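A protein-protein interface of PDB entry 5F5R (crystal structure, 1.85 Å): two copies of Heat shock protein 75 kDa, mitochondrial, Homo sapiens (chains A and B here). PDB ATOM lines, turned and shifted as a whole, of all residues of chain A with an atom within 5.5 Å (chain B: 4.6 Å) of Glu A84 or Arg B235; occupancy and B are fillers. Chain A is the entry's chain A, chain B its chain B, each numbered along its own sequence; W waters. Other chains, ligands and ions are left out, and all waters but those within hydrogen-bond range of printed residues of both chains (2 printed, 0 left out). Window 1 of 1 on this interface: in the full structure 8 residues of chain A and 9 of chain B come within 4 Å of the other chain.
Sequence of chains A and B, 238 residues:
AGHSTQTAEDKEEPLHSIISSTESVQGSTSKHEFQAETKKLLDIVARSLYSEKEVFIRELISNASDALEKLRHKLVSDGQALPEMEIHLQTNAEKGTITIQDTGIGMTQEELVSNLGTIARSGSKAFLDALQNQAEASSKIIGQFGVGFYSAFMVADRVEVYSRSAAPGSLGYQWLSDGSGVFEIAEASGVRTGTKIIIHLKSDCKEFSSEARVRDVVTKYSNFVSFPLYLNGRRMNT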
ATOM      1  N   LEU A  68     -18.680 -17.487  26.153  1.00  0.00           N
ATOM      2  CA  LEU A  68     -17.357 -17.012  25.766  1.00  0.00           C
ATOM      3  C   LEU A  68     -17.186 -15.539  26.124  1.00  0.00           C
ATOM      4  O   LEU A  68     -16.138 -15.132  26.615  1.00  0.00           O
ATOM      5  CB  LEU A  68     -17.116 -17.230  24.268  1.00  0.00           C
ATOM      6  CG  LEU A  68     -16.920 -18.695  23.862  1.00  0.00           C
ATOM      7  CD1 LEU A  68     -17.130 -18.880  22.357  1.00  0.00           C
ATOM      8  CD2 LEU A  68     -15.538 -19.186  24.276  1.00  0.00           C
ATOM      9  N   LEU A  71     -16.338 -15.327  29.755  1.00  0.00           N
ATOM     10  CA  LEU A  71     -14.928 -15.618  29.984  1.00  0.00           C
ATOM     11  C   LEU A  71     -14.038 -14.390  29.790  1.00  0.00           C
ATOM     12  O   LEU A  71     -13.063 -14.209  30.515  1.00  0.00           O
ATOM     13  CB  LEU A  71     -14.456 -16.769  29.088  1.00  0.00           C
ATOM     14  CG  LEU A  71     -13.060 -17.320  29.384  1.00  0.00           C
ATOM     15  CD1 LEU A  71     -12.988 -17.874  30.802  1.00  0.00           C
ATOM     16  CD2 LEU A  71     -12.681 -18.389  28.364  1.00  0.00           C
ATOM     17  N   GLN A  80       0.081 -14.161  31.045  1.00  0.00           N
ATOM     18  CA  GLN A  80       0.328 -15.394  30.306  1.00  0.00           C
ATOM     19  C   GLN A  80      -0.364 -15.392  28.947  1.00  0.00           C
ATOM     20  O   GLN A  80      -0.668 -14.333  28.394  1.00  0.00           O
ATOM     21  CB  GLN A  80      -0.119 -16.609  31.122  1.00  0.00           C
ATOM     22  CG  GLN A  80      -1.621 -16.698  31.337  1.00  0.00           C
ATOM     23  CD  GLN A  80      -2.009 -16.550  32.796  1.00  0.00           C
ATOM     24  OE1 GLN A  80      -1.184 -16.730  33.690  1.00  0.00           O
ATOM     25  NE2 GLN A  80      -3.269 -16.207  33.042  1.00  0.00           N
ATOM     26  N   ALA A  81      -0.488 -16.577  28.359  1.00  0.00           N
ATOM     27  CA  ALA A  81      -1.308 -16.762  27.172  1.00  0.00           C
ATOM     28  C   ALA A  81      -2.763 -16.415  27.462  1.00  0.00           C
ATOM     29  O   ALA A  81      -3.180 -16.356  28.618  1.00  0.00           O
ATOM     30  CB  ALA A  81      -1.196 -18.192  26.668  1.00  0.00           C
ATOM     31  N   LEU A  82      -3.555 -16.310  26.401  1.00  0.00           N
ATOM     32  CA  LEU A  82      -4.998 -16.177  26.533  1.00  0.00           C
ATOM     33  C   LEU A  82      -5.686 -17.499  26.220  1.00  0.00           C
ATOM     34  O   LEU A  82      -5.122 -18.338  25.516  1.00  0.00           O
ATOM     35  CB  LEU A  82      -5.503 -15.077  25.599  1.00  0.00           C
ATOM     36  CG  LEU A  82      -4.962 -13.682  25.918  1.00  0.00           C
ATOM     37  CD1 LEU A  82      -5.338 -12.696  24.824  1.00  0.00           C
ATOM     38  CD2 LEU A  82      -5.489 -13.214  27.269  1.00  0.00           C
ATOM     39  N   PRO A  83      -6.832 -17.756  26.870  1.00  0.00           N
ATOM     40  CA  PRO A  83      -7.602 -18.963  26.588  1.00  0.00           C
ATOM     41  C   PRO A  83      -8.135 -18.957  25.160  1.00  0.00           C
ATOM     42  O   PRO A  83      -8.332 -17.892  24.582  1.00  0.00           O
ATOM     43  CB  PRO A  83      -8.762 -18.871  27.582  1.00  0.00           C
ATOM     44  CG  PRO A  83      -8.946 -17.408  27.787  1.00  0.00           C
ATOM     45  CD  PRO A  83      -7.561 -16.828  27.750  1.00  0.00           C
ATOM     46  N   GLU A  84      -8.232 -20.135  24.553  1.00  0.00           N
ATOM     47  CA  GLU A  84      -8.878 -20.257  23.253  1.00  0.00           C
ATOM     48  C   GLU A  84     -10.379 -20.027  23.387  1.00  0.00           C
ATOM     49  O   GLU A  84     -10.981 -20.395  24.396  1.00  0.00           O
ATOM     50  CB  GLU A  84      -8.607 -21.636  22.644  1.00  0.00           C
ATOM     51  CG  GLU A  84      -8.222 -21.596  21.171  1.00  0.00           C
ATOM     52  CD  GLU A  84      -6.956 -20.799  20.915  1.00  0.00           C
ATOM     53  OE1 GLU A  84      -6.947 -19.976  19.974  1.00  0.00           O
ATOM     54  OE2 GLU A  84      -5.977 -20.978  21.670  1.00  0.00           O
ATOM     55  N   MET A  85     -10.942 -19.275  22.450  1.00  0.00           N
ATOM     56  CA  MET A  85     -12.338 -18.866  22.548  1.00  0.00           C
ATOM     57  C   MET A  85     -13.107 -19.181  21.266  1.00  0.00           C
ATOM     58  O   MET A  85     -12.999 -18.453  20.276  1.00  0.00           O
ATOM     59  CB  MET A  85     -12.435 -17.380  22.922  1.00  0.00           C
ATOM     60  CG  MET A  85     -12.155 -17.118  24.401  1.00  0.00           C
ATOM     61  SD  MET A  85     -12.085 -15.374  24.837  1.00  0.00           S
ATOM     62  CE  MET A  85     -10.402 -14.972  24.372  1.00  0.00           C
ATOM     63  N   GLU A  86     -13.648 -20.397  21.211  1.00  0.00           N
ATOM     64  CA  GLU A  86     -14.202 -20.957  19.977  1.00  0.00           C
ATOM     65  C   GLU A  86     -15.527 -21.667  20.238  1.00  0.00           C
ATOM     66  O   GLU A  86     -15.757 -22.192  21.330  1.00  0.00           O
ATOM     67  CB  GLU A  86     -13.219 -21.950  19.341  1.00  0.00           C
ATOM     68  CG  GLU A  86     -11.763 -21.530  19.404  1.00  0.00           C
ATOM     69  CD  GLU A  86     -10.849 -22.460  18.618  1.00  0.00           C
ATOM     70  OE1 GLU A  86     -11.224 -23.631  18.402  1.00  0.00           O
ATOM     71  OE2 GLU A  86      -9.827 -21.973  18.091  1.00  0.00           O
ATOM     72  N   THR A 103     -15.667 -23.092  24.488  1.00  0.00           N
ATOM     73  CA  THR A 103     -14.555 -23.058  25.426  1.00  0.00           C
ATOM     74  C   THR A 103     -14.679 -21.860  26.365  1.00  0.00           C
ATOM     75  O   THR A 103     -13.676 -21.293  26.801  1.00  0.00           O
ATOM     76  CB  THR A 103     -13.206 -23.013  24.688  1.00  0.00           C
ATOM     77  OG1 THR A 103     -13.143 -21.836  23.875  1.00  0.00           O
ATOM     78  CG2 THR A 103     -13.050 -24.249  23.798  1.00  0.00           C
ATOM     79  N   ARG A 192     -13.258 -30.552  29.403  1.00  0.00           N
ATOM     80  CA  ARG A 192     -12.594 -29.283  29.137  1.00  0.00           C
ATOM     81  C   ARG A 192     -13.384 -28.117  29.721  1.00  0.00           C
ATOM     82  O   ARG A 192     -14.613 -28.146  29.764  1.00  0.00           O
ATOM     83  CB  ARG A 192     -12.391 -29.085  27.634  1.00  0.00           C
ATOM     84  CG  ARG A 192     -11.532 -27.882  27.296  1.00  0.00           C
ATOM     85  CD  ARG A 192     -11.360 -27.710  25.799  1.00  0.00           C
ATOM     86  NE  ARG A 192     -10.609 -26.498  25.489  1.00  0.00           N
ATOM     87  CZ  ARG A 192      -9.886 -26.324  24.388  1.00  0.00           C
ATOM     88  NH1 ARG A 192      -9.765 -27.311  23.510  1.00  0.00           N
ATOM     89  NH2 ARG A 192      -9.259 -25.173  24.182  1.00  0.00           N
ATOM     90  N   PRO B 228      -5.222 -13.184  14.819  1.00  0.00           N
ATOM     91  CA  PRO B 228      -4.738 -14.017  15.913  1.00  0.00           C
ATOM     92  C   PRO B 228      -3.230 -14.217  15.843  1.00  0.00           C
ATOM     93  O   PRO B 228      -2.698 -14.633  14.809  1.00  0.00           O
ATOM     94  CB  PRO B 228      -5.460 -15.347  15.689  1.00  0.00           C
ATOM     95  CG  PRO B 228      -6.742 -14.955  15.032  1.00  0.00           C
ATOM     96  CD  PRO B 228      -6.405 -13.767  14.159  1.00  0.00           C
ATOM     97  N   LEU B 229      -2.561 -13.965  16.961  1.00  0.00           N
ATOM     98  CA  LEU B 229      -1.111 -14.035  17.024  1.00  0.00           C
ATOM     99  C   LEU B 229      -0.704 -15.063  18.069  1.00  0.00           C
ATOM    100  O   LEU B 229      -1.138 -14.988  19.217  1.00  0.00           O
ATOM    101  CB  LEU B 229      -0.543 -12.668  17.410  1.00  0.00           C
ATOM    102  CG  LEU B 229       0.962 -12.636  17.677  1.00  0.00           C
ATOM    103  CD1 LEU B 229       1.721 -12.833  16.373  1.00  0.00           C
ATOM    104  CD2 LEU B 229       1.346 -11.316  18.332  1.00  0.00           C
ATOM    105  N   TYR B 230       0.103 -16.036  17.655  1.00  0.00           N
ATOM    106  CA  TYR B 230       0.546 -17.100  18.550  1.00  0.00           C
ATOM    107  C   TYR B 230       2.056 -17.060  18.731  1.00  0.00           C
ATOM    108  O   TYR B 230       2.796 -16.814  17.778  1.00  0.00           O
ATOM    109  CB  TYR B 230       0.128 -18.465  18.005  1.00  0.00           C
ATOM    110  CG  TYR B 230      -1.365 -18.641  17.898  1.00  0.00           C
ATOM    111  CD1 TYR B 230      -2.089 -19.257  18.913  1.00  0.00           C
ATOM    112  CD2 TYR B 230      -2.058 -18.165  16.794  1.00  0.00           C
ATOM    113  CE1 TYR B 230      -3.461 -19.391  18.830  1.00  0.00           C
ATOM    114  CE2 TYR B 230      -3.429 -18.267  16.715  1.00  0.00           C
ATOM    115  CZ  TYR B 230      -4.124 -18.896  17.725  1.00  0.00           C
ATOM    116  OH  TYR B 230      -5.495 -18.941  17.669  1.00  0.00           O
ATOM    117  N   GLY B 233       2.670 -21.562  20.149  1.00  0.00           N
ATOM    118  CA  GLY B 233       1.398 -22.243  20.351  1.00  0.00           C
ATOM    119  C   GLY B 233       0.473 -21.529  21.321  1.00  0.00           C
ATOM    120  O   GLY B 233      -0.649 -21.974  21.556  1.00  0.00           O
ATOM    121  N   ARG B 234       0.974 -20.470  21.950  1.00  0.00           N
ATOM    122  CA  ARG B 234       0.191 -19.725  22.934  1.00  0.00           C
ATOM    123  C   ARG B 234      -0.384 -18.445  22.333  1.00  0.00           C
ATOM    124  O   ARG B 234       0.345 -17.640  21.752  1.00  0.00           O
ATOM    125  CB  ARG B 234       1.044 -19.387  24.160  1.00  0.00           C
ATOM    126  CG  ARG B 234       1.634 -20.601  24.865  1.00  0.00           C
ATOM    127  CD  ARG B 234       2.235 -20.218  26.212  1.00  0.00           C
ATOM    128  NE  ARG B 234       3.176 -21.222  26.700  1.00  0.00           N
ATOM    129  CZ  ARG B 234       2.906 -22.521  26.787  1.00  0.00           C
ATOM    130  NH1 ARG B 234       1.737 -22.985  26.369  1.00  0.00           N
ATOM    131  NH2 ARG B 234       3.821 -23.360  27.252  1.00  0.00           N
ATOM    132  N   ARG B 235      -1.680 -18.228  22.536  1.00  0.00           N
ATOM    133  CA  ARG B 235      -2.357 -17.067  21.968  1.00  0.00           C
ATOM    134  C   ARG B 235      -1.995 -15.788  22.718  1.00  0.00           C
ATOM    135  O   ARG B 235      -2.041 -15.744  23.951  1.00  0.00           O
ATOM    136  CB  ARG B 235      -3.874 -17.278  21.971  1.00  0.00           C
ATOM    137  CG  ARG B 235      -4.670 -16.092  21.450  1.00  0.00           C
ATOM    138  CD  ARG B 235      -4.570 -15.969  19.930  1.00  0.00           C
ATOM    139  NE  ARG B 235      -5.458 -14.935  19.406  1.00  0.00           N
ATOM    140  CZ  ARG B 235      -6.693 -15.160  18.963  1.00  0.00           C
ATOM    141  NH1 ARG B 235      -7.178 -16.393  18.941  1.00  0.00           N
ATOM    142  NH2 ARG B 235      -7.490 -14.141  18.679  1.00  0.00           N
ATOM    143  N   MET B 236      -1.630 -14.750  21.968  1.00  0.00           N
ATOM    144  CA  MET B 236      -1.075 -13.534  22.558  1.00  0.00           C
ATOM    145  C   MET B 236      -2.066 -12.376  22.602  1.00  0.00           C
ATOM    146  O   MET B 236      -1.819 -11.377  23.278  1.00  0.00           O
ATOM    147  CB  MET B 236       0.197 -13.097  21.827  1.00  0.00           C
ATOM    148  CG  MET B 236       1.309 -14.127  21.834  1.00  0.00           C
ATOM    149  SD  MET B 236       1.955 -14.445  23.487  1.00  0.00           S
ATOM    150  CE  MET B 236       2.763 -12.885  23.837  1.00  0.00           C
ATOM    151  N   ASN B 237      -3.104 -12.439  21.771  1.00  0.00           N
ATOM    152  CA  ASN B 237      -4.059 -11.338  21.681  1.00  0.00           C
ATOM    153  C   ASN B 237      -5.516 -11.799  21.681  1.00  0.00           C
ATOM    154  O   ASN B 237      -5.800 -12.988  21.539  1.00  0.00           O
ATOM    155  CB  ASN B 237      -3.778 -10.477  20.445  1.00  0.00           C
ATOM    156  CG  ASN B 237      -3.812 -11.275  19.155  1.00  0.00           C
ATOM    157  OD1 ASN B 237      -3.872 -12.505  19.175  1.00  0.00           O
ATOM    158  ND2 ASN B 237      -3.691 -10.585  18.027  1.00  0.00           N
ATOM    159  N   THR B 238      -6.427 -10.868  21.947  1.00  0.00           N
ATOM    160  CA  THR B 238      -7.849 -11.107  21.719  1.00  0.00           C
ATOM    161  C   THR B 238      -8.178 -11.083  20.231  1.00  0.00           C
ATOM    162  O   THR B 238      -9.228 -11.571  19.810  1.00  0.00           O
ATOM    163  CB  THR B 238      -8.724 -10.063  22.438  1.00  0.00           C
ATOM    164  OG1 THR B 238      -8.780  -8.866  21.654  1.00  0.00           O
ATOM    165  CG2 THR B 238      -8.157  -9.740  23.813  1.00  0.00           C
HETATM  166  O   HOH W   1      -3.328 -19.744  24.206  1.00  0.00           O
HETATM  167  O   HOH W   2      -6.697 -22.197  17.873  1.00  0.00           O
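The side-chain carboxylate (OE1) of Glu A84 lies within salt-bridge range of the guanidinium group (NH1) of Arg B235, at 3.7 Å.
The backbone carbonyl oxygen of Arg B235 is in hydrogen-bond range of the backbone NH of Leu A82.
The side-chain carboxylate (OE1) of Glu A84 lies within hydrogen-bond range of the side-chain hydroxyl (OH) of Tyr B230 (2.9 Å).
The backbone NH (N) of Leu B229 is in hydrogen-bond range of the side-chain amide oxygen (OD1) of Asn B237 (3.0 Å).
The backbone NH (N) of Met B236 is in hydrogen-bond range of the backbone carbonyl oxygen (O) of Leu B229 (2.8 Å).
The backbone carbonyl oxygen (O) of Glu A84 sits at hydrogen-bond distance from the side-chain hydroxyl (OG1) of Thr A103 (2.6 Å).
NE of Arg B235 is in hydrogen-bond range of O of Asn B237 (2.9 Å).
The guanidinium group (NH2) of Arg B235 sits at hydrogen-bond distance from the backbone carbonyl oxygen (O) of Thr B238 (3.3 Å).
OH of Tyr B230 is in hydrogen-bond range of NH1 of Arg B235 (3.3 Å).
Among the printed residues, merely in contact across the chains: Ala A81 with Arg B234 (3.6 Å), Ala A81 with Arg B235 (3.5 Å), Leu A82 with Met B236 (3.97 Å), Leu A82 with Asn B237 (3.3 Å) and Leu A82 with Thr B238 (3.6 Å).
Printed residues of chain B within 4 Å of Glu A84: Tyr B230 and Arg B235.
Of the printed residues of chain A, Met B236 touches Leu A82.
Of the printed residues of chain A, Tyr B230 touches Glu A84.
Gln A80 touches none of the printed residues of chain B.
Leu B229 touches none of the printed residues of chain A.
The nearest residue of chain A that does not touch Arg B235 is Gln A80 (4.9 Å).
Hydrophobic or aromatic side chains of chain A that line the printed part of chain B: Ala A81 and Leu A82.
Along chain A the printed residues that touch a printed residue of chain B span positions 81 to 84.
No position is printed for both chains.
Of the 8 pairs that touch across the chains among the printed residues, none has its exchanged pair printed and touching as well.
Water W1 bridges the backbone carbonyl oxygen (O) of Leu A82 (2.6 Å) and the backbone NH (N) of Arg B235 (2.8 Å).
Water W2 lies within hydrogen-bond range of the side-chain carboxylate (OE1) of Glu A84 (3.1 Å), the side-chain carboxylate (OE2) of Glu A86 (3.1 Å) and the side-chain hydroxyl (OH) of Tyr B230 (3.5 Å).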
